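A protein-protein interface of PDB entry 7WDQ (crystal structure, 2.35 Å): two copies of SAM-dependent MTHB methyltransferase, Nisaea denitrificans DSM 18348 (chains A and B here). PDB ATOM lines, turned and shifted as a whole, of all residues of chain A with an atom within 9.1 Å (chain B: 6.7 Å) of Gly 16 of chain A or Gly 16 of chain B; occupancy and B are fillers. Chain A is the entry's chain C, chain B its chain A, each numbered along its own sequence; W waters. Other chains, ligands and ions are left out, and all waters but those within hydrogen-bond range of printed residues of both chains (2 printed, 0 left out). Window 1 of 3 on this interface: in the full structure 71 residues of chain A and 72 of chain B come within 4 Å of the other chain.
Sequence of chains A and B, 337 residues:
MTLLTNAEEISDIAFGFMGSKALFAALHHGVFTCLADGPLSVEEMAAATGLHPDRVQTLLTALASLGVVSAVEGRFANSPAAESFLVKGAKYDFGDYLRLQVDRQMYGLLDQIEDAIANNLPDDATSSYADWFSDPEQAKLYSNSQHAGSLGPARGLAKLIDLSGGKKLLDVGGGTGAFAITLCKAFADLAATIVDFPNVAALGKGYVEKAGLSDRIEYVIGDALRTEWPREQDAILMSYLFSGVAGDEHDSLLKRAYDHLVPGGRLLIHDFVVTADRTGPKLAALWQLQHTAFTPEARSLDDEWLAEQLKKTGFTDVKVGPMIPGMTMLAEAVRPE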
ATOM      1  N   GLU A   8      23.247  19.967 -21.178  1.00  0.00           N
ATOM      2  CA  GLU A   8      22.576  18.914 -21.932  1.00  0.00           C
ATOM      3  C   GLU A   8      21.765  18.004 -21.001  1.00  0.00           C
ATOM      4  O   GLU A   8      20.603  17.716 -21.265  1.00  0.00           O
ATOM      5  CB  GLU A   8      23.594  18.108 -22.764  1.00  0.00           C
ATOM      6  CG  GLU A   8      22.979  17.086 -23.726  1.00  0.00           C
ATOM      7  CD  GLU A   8      24.027  16.307 -24.528  1.00  0.00           C
ATOM      8  OE1 GLU A   8      25.227  16.350 -24.163  1.00  0.00           O
ATOM      9  OE2 GLU A   8      23.654  15.651 -25.528  1.00  0.00           O
ATOM     10  N   GLU A   9      22.380  17.581 -19.902  1.00  0.00           N
ATOM     11  CA  GLU A   9      21.757  16.652 -18.962  1.00  0.00           C
ATOM     12  C   GLU A   9      20.552  17.261 -18.242  1.00  0.00           C
ATOM     13  O   GLU A   9      19.570  16.567 -17.956  1.00  0.00           O
ATOM     14  CB  GLU A   9      22.795  16.137 -17.960  1.00  0.00           C
ATOM     15  CG  GLU A   9      23.945  15.375 -18.629  1.00  0.00           C
ATOM     16  CD  GLU A   9      25.119  15.065 -17.690  1.00  0.00           C
ATOM     17  OE1 GLU A   9      25.237  15.728 -16.638  1.00  0.00           O
ATOM     18  OE2 GLU A   9      25.927  14.158 -18.020  1.00  0.00           O
ATOM     19  N   ILE A  10      20.617  18.556 -17.956  1.00  0.00           N
ATOM     20  CA  ILE A  10      19.464  19.217 -17.360  1.00  0.00           C
ATOM     21  C   ILE A  10      18.387  19.477 -18.408  1.00  0.00           C
ATOM     22  O   ILE A  10      17.219  19.230 -18.160  1.00  0.00           O
ATOM     23  CB  ILE A  10      19.832  20.517 -16.624  1.00  0.00           C
ATOM     24  CG1 ILE A  10      20.274  20.198 -15.206  1.00  0.00           C
ATOM     25  CG2 ILE A  10      18.592  21.387 -16.460  1.00  0.00           C
ATOM     26  CD1 ILE A  10      19.087  20.067 -14.270  1.00  0.00           C
ATOM     27  N   SER A  11      18.777  19.963 -19.579  1.00  0.00           N
ATOM     28  CA  SER A  11      17.826  20.085 -20.671  1.00  0.00           C
ATOM     29  C   SER A  11      17.113  18.761 -20.882  1.00  0.00           C
ATOM     30  O   SER A  11      15.906  18.739 -21.070  1.00  0.00           O
ATOM     31  CB  SER A  11      18.504  20.509 -21.974  1.00  0.00           C
ATOM     32  OG  SER A  11      19.130  21.769 -21.832  1.00  0.00           O
ATOM     33  N   ASP A  12      17.848  17.654 -20.841  1.00  0.00           N
ATOM     34  CA  ASP A  12      17.232  16.361 -21.096  1.00  0.00           C
ATOM     35  C   ASP A  12      16.056  16.156 -20.158  1.00  0.00           C
ATOM     36  O   ASP A  12      15.021  15.642 -20.580  1.00  0.00           O
ATOM     37  CB  ASP A  12      18.230  15.210 -20.949  1.00  0.00           C
ATOM     38  CG  ASP A  12      19.162  15.075 -22.152  1.00  0.00           C
ATOM     39  OD1 ASP A  12      18.748  15.438 -23.281  1.00  0.00           O
ATOM     40  OD2 ASP A  12      20.309  14.594 -21.963  1.00  0.00           O
ATOM     41  N   ILE A  13      16.223  16.557 -18.892  1.00  0.00           N
ATOM     42  CA  ILE A  13      15.150  16.469 -17.898  1.00  0.00           C
ATOM     43  C   ILE A  13      14.051  17.497 -18.177  1.00  0.00           C
ATOM     44  O   ILE A  13      12.868  17.157 -18.240  1.00  0.00           O
ATOM     45  CB  ILE A  13      15.654  16.719 -16.442  1.00  0.00           C
ATOM     46  CG1 ILE A  13      16.770  15.747 -16.047  1.00  0.00           C
ATOM     47  CG2 ILE A  13      14.506  16.629 -15.467  1.00  0.00           C
ATOM     48  CD1 ILE A  13      16.455  14.278 -16.339  1.00  0.00           C
ATOM     49  N   ALA A  14      14.449  18.763 -18.315  1.00  0.00           N
ATOM     50  CA  ALA A  14      13.493  19.851 -18.490  1.00  0.00           C
ATOM     51  C   ALA A  14      12.572  19.614 -19.688  1.00  0.00           C
ATOM     52  O   ALA A  14      11.380  19.869 -19.607  1.00  0.00           O
ATOM     53  CB  ALA A  14      14.212  21.194 -18.625  1.00  0.00           C
ATOM     54  N   PHE A  15      13.119  19.100 -20.788  1.00  0.00           N
ATOM     55  CA  PHE A  15      12.339  18.927 -22.006  1.00  0.00           C
ATOM     56  C   PHE A  15      11.865  17.487 -22.251  1.00  0.00           C
ATOM     57  O   PHE A  15      11.340  17.166 -23.311  1.00  0.00           O
ATOM     58  CB  PHE A  15      13.093  19.528 -23.189  1.00  0.00           C
ATOM     59  CG  PHE A  15      13.401  20.989 -22.996  1.00  0.00           C
ATOM     60  CD1 PHE A  15      12.369  21.907 -22.831  1.00  0.00           C
ATOM     61  CD2 PHE A  15      14.698  21.444 -22.940  1.00  0.00           C
ATOM     62  CE1 PHE A  15      12.632  23.248 -22.617  1.00  0.00           C
ATOM     63  CE2 PHE A  15      14.969  22.793 -22.740  1.00  0.00           C
ATOM     64  CZ  PHE A  15      13.936  23.693 -22.583  1.00  0.00           C
ATOM     65  N   GLY A  16      12.006  16.632 -21.246  1.00  0.00           N
ATOM     66  CA  GLY A  16      11.441  15.296 -21.331  1.00  0.00           C
ATOM     67  C   GLY A  16       9.949  15.258 -21.675  1.00  0.00           C
ATOM     68  O   GLY A  16       9.484  14.316 -22.318  1.00  0.00           O
ATOM     69  N   PHE A  17       9.179  16.254 -21.230  1.00  0.00           N
ATOM     70  CA  PHE A  17       7.747  16.245 -21.512  1.00  0.00           C
ATOM     71  C   PHE A  17       7.498  16.330 -23.021  1.00  0.00           C
ATOM     72  O   PHE A  17       6.533  15.798 -23.527  1.00  0.00           O
ATOM     73  CB  PHE A  17       6.977  17.341 -20.733  1.00  0.00           C
ATOM     74  CG  PHE A  17       7.236  18.752 -21.223  1.00  0.00           C
ATOM     75  CD1 PHE A  17       8.321  19.487 -20.743  1.00  0.00           C
ATOM     76  CD2 PHE A  17       6.393  19.343 -22.150  1.00  0.00           C
ATOM     77  CE1 PHE A  17       8.567  20.789 -21.187  1.00  0.00           C
ATOM     78  CE2 PHE A  17       6.630  20.642 -22.599  1.00  0.00           C
ATOM     79  CZ  PHE A  17       7.722  21.361 -22.127  1.00  0.00           C
ATOM     80  N   MET A  18       8.377  16.979 -23.754  1.00  0.00           N
ATOM     81  CA  MET A  18       8.152  17.059 -25.184  1.00  0.00           C
ATOM     82  C   MET A  18       8.343  15.696 -25.810  1.00  0.00           C
ATOM     83  O   MET A  18       7.562  15.288 -26.683  1.00  0.00           O
ATOM     84  CB  MET A  18       9.060  18.107 -25.823  1.00  0.00           C
ATOM     85  CG  MET A  18       8.900  19.483 -25.178  1.00  0.00           C
ATOM     86  SD  MET A  18       9.926  20.690 -26.025  1.00  0.00           S
ATOM     87  CE  MET A  18       9.488  22.221 -25.199  1.00  0.00           C
ATOM     88  N   GLY A  19       9.377  14.985 -25.344  1.00  0.00           N
ATOM     89  CA  GLY A  19       9.608  13.617 -25.746  1.00  0.00           C
ATOM     90  C   GLY A  19       8.374  12.763 -25.534  1.00  0.00           C
ATOM     91  O   GLY A  19       7.917  12.086 -26.461  1.00  0.00           O
ATOM     92  N   SER A  20       7.822  12.804 -24.323  1.00  0.00           N
ATOM     93  CA  SER A  20       6.646  11.996 -23.994  1.00  0.00           C
ATOM     94  C   SER A  20       5.498  12.261 -24.956  1.00  0.00           C
ATOM     95  O   SER A  20       4.851  11.325 -25.441  1.00  0.00           O
ATOM     96  CB  SER A  20       6.180  12.267 -22.566  1.00  0.00           C
ATOM     97  OG  SER A  20       7.237  12.090 -21.644  1.00  0.00           O
ATOM     98  N   LYS A  21       5.275  13.539 -25.256  1.00  0.00           N
ATOM     99  CA  LYS A  21       4.139  13.945 -26.097  1.00  0.00           C
ATOM    100  C   LYS A  21       4.319  13.556 -27.549  1.00  0.00           C
ATOM    101  O   LYS A  21       3.331  13.326 -28.254  1.00  0.00           O
ATOM    102  CB  LYS A  21       3.853  15.455 -25.987  1.00  0.00           C
ATOM    103  CG  LYS A  21       2.951  15.817 -24.827  1.00  0.00           C
ATOM    104  CD  LYS A  21       1.559  15.218 -25.036  1.00  0.00           C
ATOM    105  CE  LYS A  21       0.545  15.771 -24.051  1.00  0.00           C
ATOM    106  NZ  LYS A  21      -0.824  15.266 -24.340  1.00  0.00           N
ATOM    107  N   ALA A  22       5.570  13.501 -28.001  1.00  0.00           N
ATOM    108  CA  ALA A  22       5.855  13.040 -29.361  1.00  0.00           C
ATOM    109  C   ALA A  22       5.401  11.589 -29.514  1.00  0.00           C
ATOM    110  O   ALA A  22       4.812  11.201 -30.507  1.00  0.00           O
ATOM    111  CB  ALA A  22       7.330  13.154 -29.652  1.00  0.00           C
ATOM    112  N   LEU A  23       5.700  10.789 -28.508  1.00  0.00           N
ATOM    113  CA  LEU A  23       5.362   9.383 -28.509  1.00  0.00           C
ATOM    114  C   LEU A  23       3.833   9.215 -28.462  1.00  0.00           C
ATOM    115  O   LEU A  23       3.265   8.447 -29.235  1.00  0.00           O
ATOM    116  CB  LEU A  23       6.048   8.707 -27.304  1.00  0.00           C
ATOM    117  CG  LEU A  23       5.673   7.274 -26.942  1.00  0.00           C
ATOM    118  CD1 LEU A  23       5.920   6.402 -28.145  1.00  0.00           C
ATOM    119  CD2 LEU A  23       6.464   6.767 -25.729  1.00  0.00           C
ATOM    120  N   PHE A  24       3.180   9.956 -27.567  1.00  0.00           N
ATOM    121  CA  PHE A  24       1.728   9.908 -27.408  1.00  0.00           C
ATOM    122  C   PHE A  24       0.960  10.325 -28.661  1.00  0.00           C
ATOM    123  O   PHE A  24       0.091   9.594 -29.133  1.00  0.00           O
ATOM    124  CB  PHE A  24       1.302  10.764 -26.223  1.00  0.00           C
ATOM    125  CG  PHE A  24       1.916  10.332 -24.938  1.00  0.00           C
ATOM    126  CD1 PHE A  24       2.388   9.032 -24.789  1.00  0.00           C
ATOM    127  CD2 PHE A  24       2.049  11.222 -23.883  1.00  0.00           C
ATOM    128  CE1 PHE A  24       2.971   8.621 -23.591  1.00  0.00           C
ATOM    129  CE2 PHE A  24       2.630  10.814 -22.685  1.00  0.00           C
ATOM    130  CZ  PHE A  24       3.090   9.512 -22.538  1.00  0.00           C
ATOM    131  N   LEU A  66      14.699  10.697 -31.144  1.00  0.00           N
ATOM    132  CA  LEU A  66      14.564   9.968 -29.887  1.00  0.00           C
ATOM    133  C   LEU A  66      14.994   8.502 -30.052  1.00  0.00           C
ATOM    134  O   LEU A  66      15.114   7.763 -29.077  1.00  0.00           O
ATOM    135  CB  LEU A  66      13.117  10.021 -29.386  1.00  0.00           C
ATOM    136  CG  LEU A  66      12.511  11.368 -28.985  1.00  0.00           C
ATOM    137  CD1 LEU A  66      11.052  11.199 -28.676  1.00  0.00           C
ATOM    138  CD2 LEU A  66      13.229  11.951 -27.766  1.00  0.00           C
ATOM    139  N   VAL A 102      -1.975   7.204 -19.508  1.00  0.00           N
ATOM    140  CA  VAL A 102      -0.829   8.048 -19.204  1.00  0.00           C
ATOM    141  C   VAL A 102      -0.913   9.412 -19.876  1.00  0.00           C
ATOM    142  O   VAL A 102      -0.650  10.436 -19.249  1.00  0.00           O
ATOM    143  CB  VAL A 102       0.495   7.388 -19.589  1.00  0.00           C
ATOM    144  CG1 VAL A 102       1.633   8.344 -19.276  1.00  0.00           C
ATOM    145  CG2 VAL A 102       0.656   6.051 -18.856  1.00  0.00           C
ATOM    146  N   TYR A 107      -1.066  13.048 -17.688  1.00  0.00           N
ATOM    147  CA  TYR A 107      -0.285  14.206 -18.100  1.00  0.00           C
ATOM    148  C   TYR A 107      -0.964  15.515 -17.684  1.00  0.00           C
ATOM    149  O   TYR A 107      -0.314  16.422 -17.136  1.00  0.00           O
ATOM    150  CB  TYR A 107      -0.103  14.176 -19.609  1.00  0.00           C
ATOM    151  CG  TYR A 107       0.694  15.325 -20.192  1.00  0.00           C
ATOM    152  CD1 TYR A 107       0.072  16.515 -20.537  1.00  0.00           C
ATOM    153  CD2 TYR A 107       2.066  15.202 -20.424  1.00  0.00           C
ATOM    154  CE1 TYR A 107       0.791  17.562 -21.083  1.00  0.00           C
ATOM    155  CE2 TYR A 107       2.802  16.242 -20.971  1.00  0.00           C
ATOM    156  CZ  TYR A 107       2.160  17.418 -21.307  1.00  0.00           C
ATOM    157  OH  TYR A 107       2.877  18.460 -21.862  1.00  0.00           O
ATOM    158  N   LEU A 110      -0.938  16.140 -13.960  1.00  0.00           N
ATOM    159  CA  LEU A 110       0.326  16.501 -13.329  1.00  0.00           C
ATOM    160  C   LEU A 110       0.517  18.020 -13.345  1.00  0.00           C
ATOM    161  O   LEU A 110       1.391  18.544 -12.669  1.00  0.00           O
ATOM    162  CB  LEU A 110       1.510  15.744 -13.948  1.00  0.00           C
ATOM    163  CG  LEU A 110       2.797  15.708 -13.113  1.00  0.00           C
ATOM    164  CD1 LEU A 110       2.502  15.309 -11.682  1.00  0.00           C
ATOM    165  CD2 LEU A 110       3.872  14.776 -13.738  1.00  0.00           C
ATOM    166  N   LYS A 282      13.531   4.797 -10.166  1.00  0.00           N
ATOM    167  CA  LYS A 282      13.037   6.005 -10.791  1.00  0.00           C
ATOM    168  C   LYS A 282      11.530   6.004 -11.029  1.00  0.00           C
ATOM    169  O   LYS A 282      10.847   6.914 -10.608  1.00  0.00           O
ATOM    170  CB  LYS A 282      13.774   6.254 -12.105  1.00  0.00           C
ATOM    171  CG  LYS A 282      13.148   7.329 -12.969  1.00  0.00           C
ATOM    172  CD  LYS A 282      13.967   7.621 -14.207  1.00  0.00           C
ATOM    173  CE  LYS A 282      13.380   6.946 -15.430  1.00  0.00           C
ATOM    174  NZ  LYS A 282      14.030   7.386 -16.692  1.00  0.00           N
ATOM    175  N   LEU A 283      11.020   5.000 -11.723  1.00  0.00           N
ATOM    176  CA  LEU A 283       9.595   4.974 -12.039  1.00  0.00           C
ATOM    177  C   LEU A 283       8.714   4.941 -10.794  1.00  0.00           C
ATOM    178  O   LEU A 283       7.595   5.447 -10.804  1.00  0.00           O
ATOM    179  CB  LEU A 283       9.249   3.796 -12.948  1.00  0.00           C
ATOM    180  CG  LEU A 283       9.897   3.851 -14.324  1.00  0.00           C
ATOM    181  CD1 LEU A 283       9.458   2.661 -15.158  1.00  0.00           C
ATOM    182  CD2 LEU A 283       9.529   5.156 -14.992  1.00  0.00           C
ATOM    183  N   LEU A 286       8.750   8.557  -9.437  1.00  0.00           N
ATOM    184  CA  LEU A 286       7.968   9.441 -10.300  1.00  0.00           C
ATOM    185  C   LEU A 286       6.477   9.194 -10.149  1.00  0.00           C
ATOM    186  O   LEU A 286       5.687  10.135 -10.136  1.00  0.00           O
ATOM    187  CB  LEU A 286       8.375   9.294 -11.767  1.00  0.00           C
ATOM    188  CG  LEU A 286       9.827   9.649 -12.136  1.00  0.00           C
ATOM    189  CD1 LEU A 286      10.133   9.281 -13.587  1.00  0.00           C
ATOM    190  CD2 LEU A 286      10.134  11.124 -11.877  1.00  0.00           C
ATOM    191  N   SER B  11       9.665   3.211 -21.964  1.00  0.00           N
ATOM    192  CA  SER B  11       9.188   3.734 -20.682  1.00  0.00           C
ATOM    193  C   SER B  11       9.857   5.039 -20.316  1.00  0.00           C
ATOM    194  O   SER B  11       9.198   5.969 -19.852  1.00  0.00           O
ATOM    195  CB  SER B  11       9.422   2.729 -19.553  1.00  0.00           C
ATOM    196  OG  SER B  11       8.214   2.090 -19.193  1.00  0.00           O
ATOM    197  N   ASP B  12      11.173   5.094 -20.513  1.00  0.00           N
ATOM    198  CA  ASP B  12      11.945   6.273 -20.148  1.00  0.00           C
ATOM    199  C   ASP B  12      11.427   7.473 -20.910  1.00  0.00           C
ATOM    200  O   ASP B  12      11.297   8.561 -20.345  1.00  0.00           O
ATOM    201  CB  ASP B  12      13.433   6.074 -20.433  1.00  0.00           C
ATOM    202  CG  ASP B  12      14.058   5.012 -19.547  1.00  0.00           C
ATOM    203  OD1 ASP B  12      13.437   4.680 -18.507  1.00  0.00           O
ATOM    204  OD2 ASP B  12      15.164   4.521 -19.892  1.00  0.00           O
ATOM    205  N   ILE B  13      11.151   7.275 -22.198  1.00  0.00           N
ATOM    206  CA  ILE B  13      10.559   8.327 -23.004  1.00  0.00           C
ATOM    207  C   ILE B  13       9.135   8.643 -22.530  1.00  0.00           C
ATOM    208  O   ILE B  13       8.840   9.791 -22.183  1.00  0.00           O
ATOM    209  CB  ILE B  13      10.551   7.970 -24.486  1.00  0.00           C
ATOM    210  CG1 ILE B  13      11.984   7.948 -25.023  1.00  0.00           C
ATOM    211  CG2 ILE B  13       9.706   8.967 -25.259  1.00  0.00           C
ATOM    212  CD1 ILE B  13      12.106   7.327 -26.404  1.00  0.00           C
ATOM    213  N   ALA B  14       8.267   7.627 -22.488  1.00  0.00           N
ATOM    214  CA  ALA B  14       6.877   7.827 -22.057  1.00  0.00           C
ATOM    215  C   ALA B  14       6.781   8.639 -20.767  1.00  0.00           C
ATOM    216  O   ALA B  14       5.939   9.521 -20.663  1.00  0.00           O
ATOM    217  CB  ALA B  14       6.131   6.483 -21.905  1.00  0.00           C
ATOM    218  N   PHE B  15       7.660   8.369 -19.801  1.00  0.00           N
ATOM    219  CA  PHE B  15       7.530   8.976 -18.479  1.00  0.00           C
ATOM    220  C   PHE B  15       8.386  10.220 -18.221  1.00  0.00           C
ATOM    221  O   PHE B  15       8.373  10.766 -17.126  1.00  0.00           O
ATOM    222  CB  PHE B  15       7.706   7.915 -17.388  1.00  0.00           C
ATOM    223  CG  PHE B  15       6.581   6.912 -17.361  1.00  0.00           C
ATOM    224  CD1 PHE B  15       5.351   7.243 -16.794  1.00  0.00           C
ATOM    225  CD2 PHE B  15       6.729   5.664 -17.940  1.00  0.00           C
ATOM    226  CE1 PHE B  15       4.300   6.335 -16.787  1.00  0.00           C
ATOM    227  CE2 PHE B  15       5.678   4.744 -17.936  1.00  0.00           C
ATOM    228  CZ  PHE B  15       4.463   5.083 -17.361  1.00  0.00           C
ATOM    229  N   GLY B  16       9.100  10.687 -19.237  1.00  0.00           N
ATOM    230  CA  GLY B  16       9.912  11.880 -19.102  1.00  0.00           C
ATOM    231  C   GLY B  16       9.129  13.070 -18.576  1.00  0.00           C
ATOM    232  O   GLY B  16       9.676  13.887 -17.831  1.00  0.00           O
ATOM    233  N   PHE B  17       7.852  13.184 -18.947  1.00  0.00           N
ATOM    234  CA  PHE B  17       7.070  14.332 -18.496  1.00  0.00           C
ATOM    235  C   PHE B  17       6.993  14.409 -16.961  1.00  0.00           C
ATOM    236  O   PHE B  17       6.947  15.494 -16.378  1.00  0.00           O
ATOM    237  CB  PHE B  17       5.675  14.349 -19.131  1.00  0.00           C
ATOM    238  CG  PHE B  17       4.734  13.332 -18.571  1.00  0.00           C
ATOM    239  CD1 PHE B  17       4.708  12.039 -19.081  1.00  0.00           C
ATOM    240  CD2 PHE B  17       3.872  13.667 -17.541  1.00  0.00           C
ATOM    241  CE1 PHE B  17       3.833  11.104 -18.588  1.00  0.00           C
ATOM    242  CE2 PHE B  17       2.987  12.745 -17.028  1.00  0.00           C
ATOM    243  CZ  PHE B  17       2.967  11.450 -17.541  1.00  0.00           C
ATOM    244  N   MET B  18       7.020  13.256 -16.306  1.00  0.00           N
ATOM    245  CA  MET B  18       7.009  13.252 -14.853  1.00  0.00           C
ATOM    246  C   MET B  18       8.313  13.807 -14.300  1.00  0.00           C
ATOM    247  O   MET B  18       8.316  14.504 -13.289  1.00  0.00           O
ATOM    248  CB  MET B  18       6.745  11.843 -14.328  1.00  0.00           C
ATOM    249  CG  MET B  18       5.442  11.256 -14.835  1.00  0.00           C
ATOM    250  SD  MET B  18       5.098   9.665 -14.076  1.00  0.00           S
ATOM    251  CE  MET B  18       3.423   9.372 -14.665  1.00  0.00           C
ATOM    252  N   GLY B  19       9.421  13.492 -14.965  1.00  0.00           N
ATOM    253  CA  GLY B  19      10.698  14.075 -14.602  1.00  0.00           C
ATOM    254  C   GLY B  19      10.686  15.591 -14.722  1.00  0.00           C
ATOM    255  O   GLY B  19      11.150  16.314 -13.814  1.00  0.00           O
ATOM    256  N   SER B  20      10.152  16.079 -15.841  1.00  0.00           N
ATOM    257  CA  SER B  20      10.149  17.516 -16.106  1.00  0.00           C
ATOM    258  C   SER B  20       9.396  18.250 -15.001  1.00  0.00           C
ATOM    259  O   SER B  20       9.841  19.292 -14.519  1.00  0.00           O
ATOM    260  CB  SER B  20       9.531  17.834 -17.477  1.00  0.00           C
ATOM    261  OG  SER B  20      10.018  16.965 -18.496  1.00  0.00           O
ATOM    262  N   LYS B  21       8.267  17.675 -14.595  1.00  0.00           N
ATOM    263  CA  LYS B  21       7.396  18.298 -13.621  1.00  0.00           C
ATOM    264  C   LYS B  21       7.989  18.233 -12.224  1.00  0.00           C
ATOM    265  O   LYS B  21       7.781  19.139 -11.422  1.00  0.00           O
ATOM    266  CB  LYS B  21       6.010  17.650 -13.627  1.00  0.00           C
ATOM    267  CG  LYS B  21       5.185  17.947 -14.867  1.00  0.00           C
ATOM    268  CD  LYS B  21       5.010  19.452 -15.112  1.00  0.00           C
ATOM    269  CE  LYS B  21       4.051  20.095 -14.132  1.00  0.00           C
ATOM    270  NZ  LYS B  21       3.320  21.277 -14.733  1.00  0.00           N
ATOM    271  N   LEU B 286      12.219  18.655 -31.000  1.00  0.00           N
ATOM    272  CA  LEU B 286      11.181  18.706 -29.971  1.00  0.00           C
ATOM    273  C   LEU B 286      10.562  20.108 -29.911  1.00  0.00           C
ATOM    274  O   LEU B 286       9.348  20.239 -29.883  1.00  0.00           O
ATOM    275  CB  LEU B 286      11.701  18.237 -28.604  1.00  0.00           C
ATOM    276  CG  LEU B 286      12.191  16.782 -28.562  1.00  0.00           C
ATOM    277  CD1 LEU B 286      12.704  16.329 -27.163  1.00  0.00           C
ATOM    278  CD2 LEU B 286      11.095  15.856 -29.083  1.00  0.00           C
HETATM  279  O   HOH W   1      12.284  14.275 -17.935  1.00  0.00           O
HETATM  280  O   HOH W   2      10.778  11.965 -22.737  1.00  0.00           O
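Of chain B, only Gly 16, Phe 17 and Ser 20 come within 4 Å of Gly 16 of chain A. Leu 66 of chain A touches none of the printed residues of chain B. Of the printed residues of chain B, Leu 286 of chain A touches Met 18 (3.96 Å) and Gly 19 (3.96 Å). Of chain A, only Gly 16 and Ser 20 come within 4 Å of Gly 16 of chain B. Of the printed residues of chain A, Met 18 of chain B touches Leu 110 (3.7 Å) and Leu 286 (3.96 Å). Of chain A, only Ile 13 (3.8 Å) and Leu 286 (3.96 Å) come within 4 Å of Gly 19 of chain B. The nearest printed residue of chain A that does not touch Ala 14 of chain B is Val 102 of chain A (4.7 Å).
Ile 13 of chain A touches Gly 19 of chain B, and with the chains exchanged Gly 19 of chain A touches Ile 13 of chain B. Phe 17 of chain A touches Ser 20 of chain B, and with the chains exchanged Ser 20 of chain A touches Phe 17 of chain B. Met 18 of chain A touches Leu 286 of chain B, and with the chains exchanged Leu 286 of chain A touches Met 18 of chain B. Leu 286 of chain A touches Gly 19 of chain B, but with the chains exchanged Gly 19 of chain A does not touch Leu 286 of chain B (4.02 Å). Of the 25 pairs that touch across the chains among the printed residues, 14 have their exchanged pair printed and touching as well.
N of Tyr 107 of chain A is in hydrogen-bond range of O of Val 102 of chain A (3.1 Å). OG of Ser 20 of chain A is in hydrogen-bond range of O of Gly 16 of chain A (3.2 Å). O of Gly 16 of chain B lies within hydrogen-bond range of OG of Ser 20 of chain B, 3.2 Å away.
Hydrophobic or aromatic side chains of chain B that line the printed part of chain A: Ile 13, Ala 14, Phe 17, Met 18 and Leu 286. Among the printed residues, 25 pairs touch across the chains.
Water W1 lies within hydrogen-bond range of O of Gly 16 of chain B (2.6 Å), O of Ile 13 of chain A (3.0 Å) and N of Ser 20 of chain B (3.5 Å). Water W2 lies within hydrogen-bond range of the backbone carbonyl oxygen (O) of Gly 16 of chain A (2.7 Å), the backbone carbonyl oxygen (O) of Ile 13 of chain B (3.0 Å) and the backbone NH (N) of Ser 20 of chain A (3.5 Å).
CB of Phe 17 of chain A touches CB of Phe 17 of chain B (3.6 Å). Met 18 of chain A touches Leu 286 of chain B (CB to CB, 3.8 Å). O of Gly 19 of chain A touches CG2 of Ile 13 of chain B, at 3.8 Å. Leu 23 of chain A touches Ile 13 of chain B. Ala 14 of chain B touches Leu 23 of chain A. Phe 17 of chain B touches Val 102 of chain A (CE1 to CG1, 3.6 Å). Tyr 107 of chain A touches Phe 17 of chain B. Leu 110 of chain A touches Phe 17 of chain B (CD2 to CD2, 3.96 Å). Leu 110 of chain A touches Lys 21 of chain B. Met 18 of chain B touches Leu 286 of chain A.
The side-chain hydroxyl (OG) of Ser 20 of chain B is in hydrogen-bond range of the backbone NH (N) of Phe 17 of chain A (2.9 Å). The backbone carbonyl oxygen of Ala 14 of chain B sits at hydrogen-bond distance from the side-chain hydroxyl of Ser 20 of chain A. O of Ala 14 of chain A sits at hydrogen-bond distance from OG of Ser 20 of chain B (3.4 Å). O of Ile 13 of chain B lies within hydrogen-bond range of OG of Ser 20 of chain A (2.9 Å). The side-chain hydroxyl (OG) of Ser 20 of chain B sits at hydrogen-bond distance from the backbone carbonyl oxygen (O) of Ile 13 of chain A. The backbone NH (N) of Phe 17 of chain B lies within hydrogen-bond range of the side-chain hydroxyl (OG) of Ser 20 of chain A (3.0 Å). N of Gly 16 of chain A is in hydrogen-bond range of OG of Ser 20 of chain B, 3.4 Å away. The backbone NH (N) of Gly 16 of chain B sits at hydrogen-bond distance from the side-chain hydroxyl (OG) of Ser 20 of chain A, at 3.4 Å. OD1 of Asp 12 of chain B lies within salt-bridge range of NZ of Lys 282 of chain A (3.3 Å).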
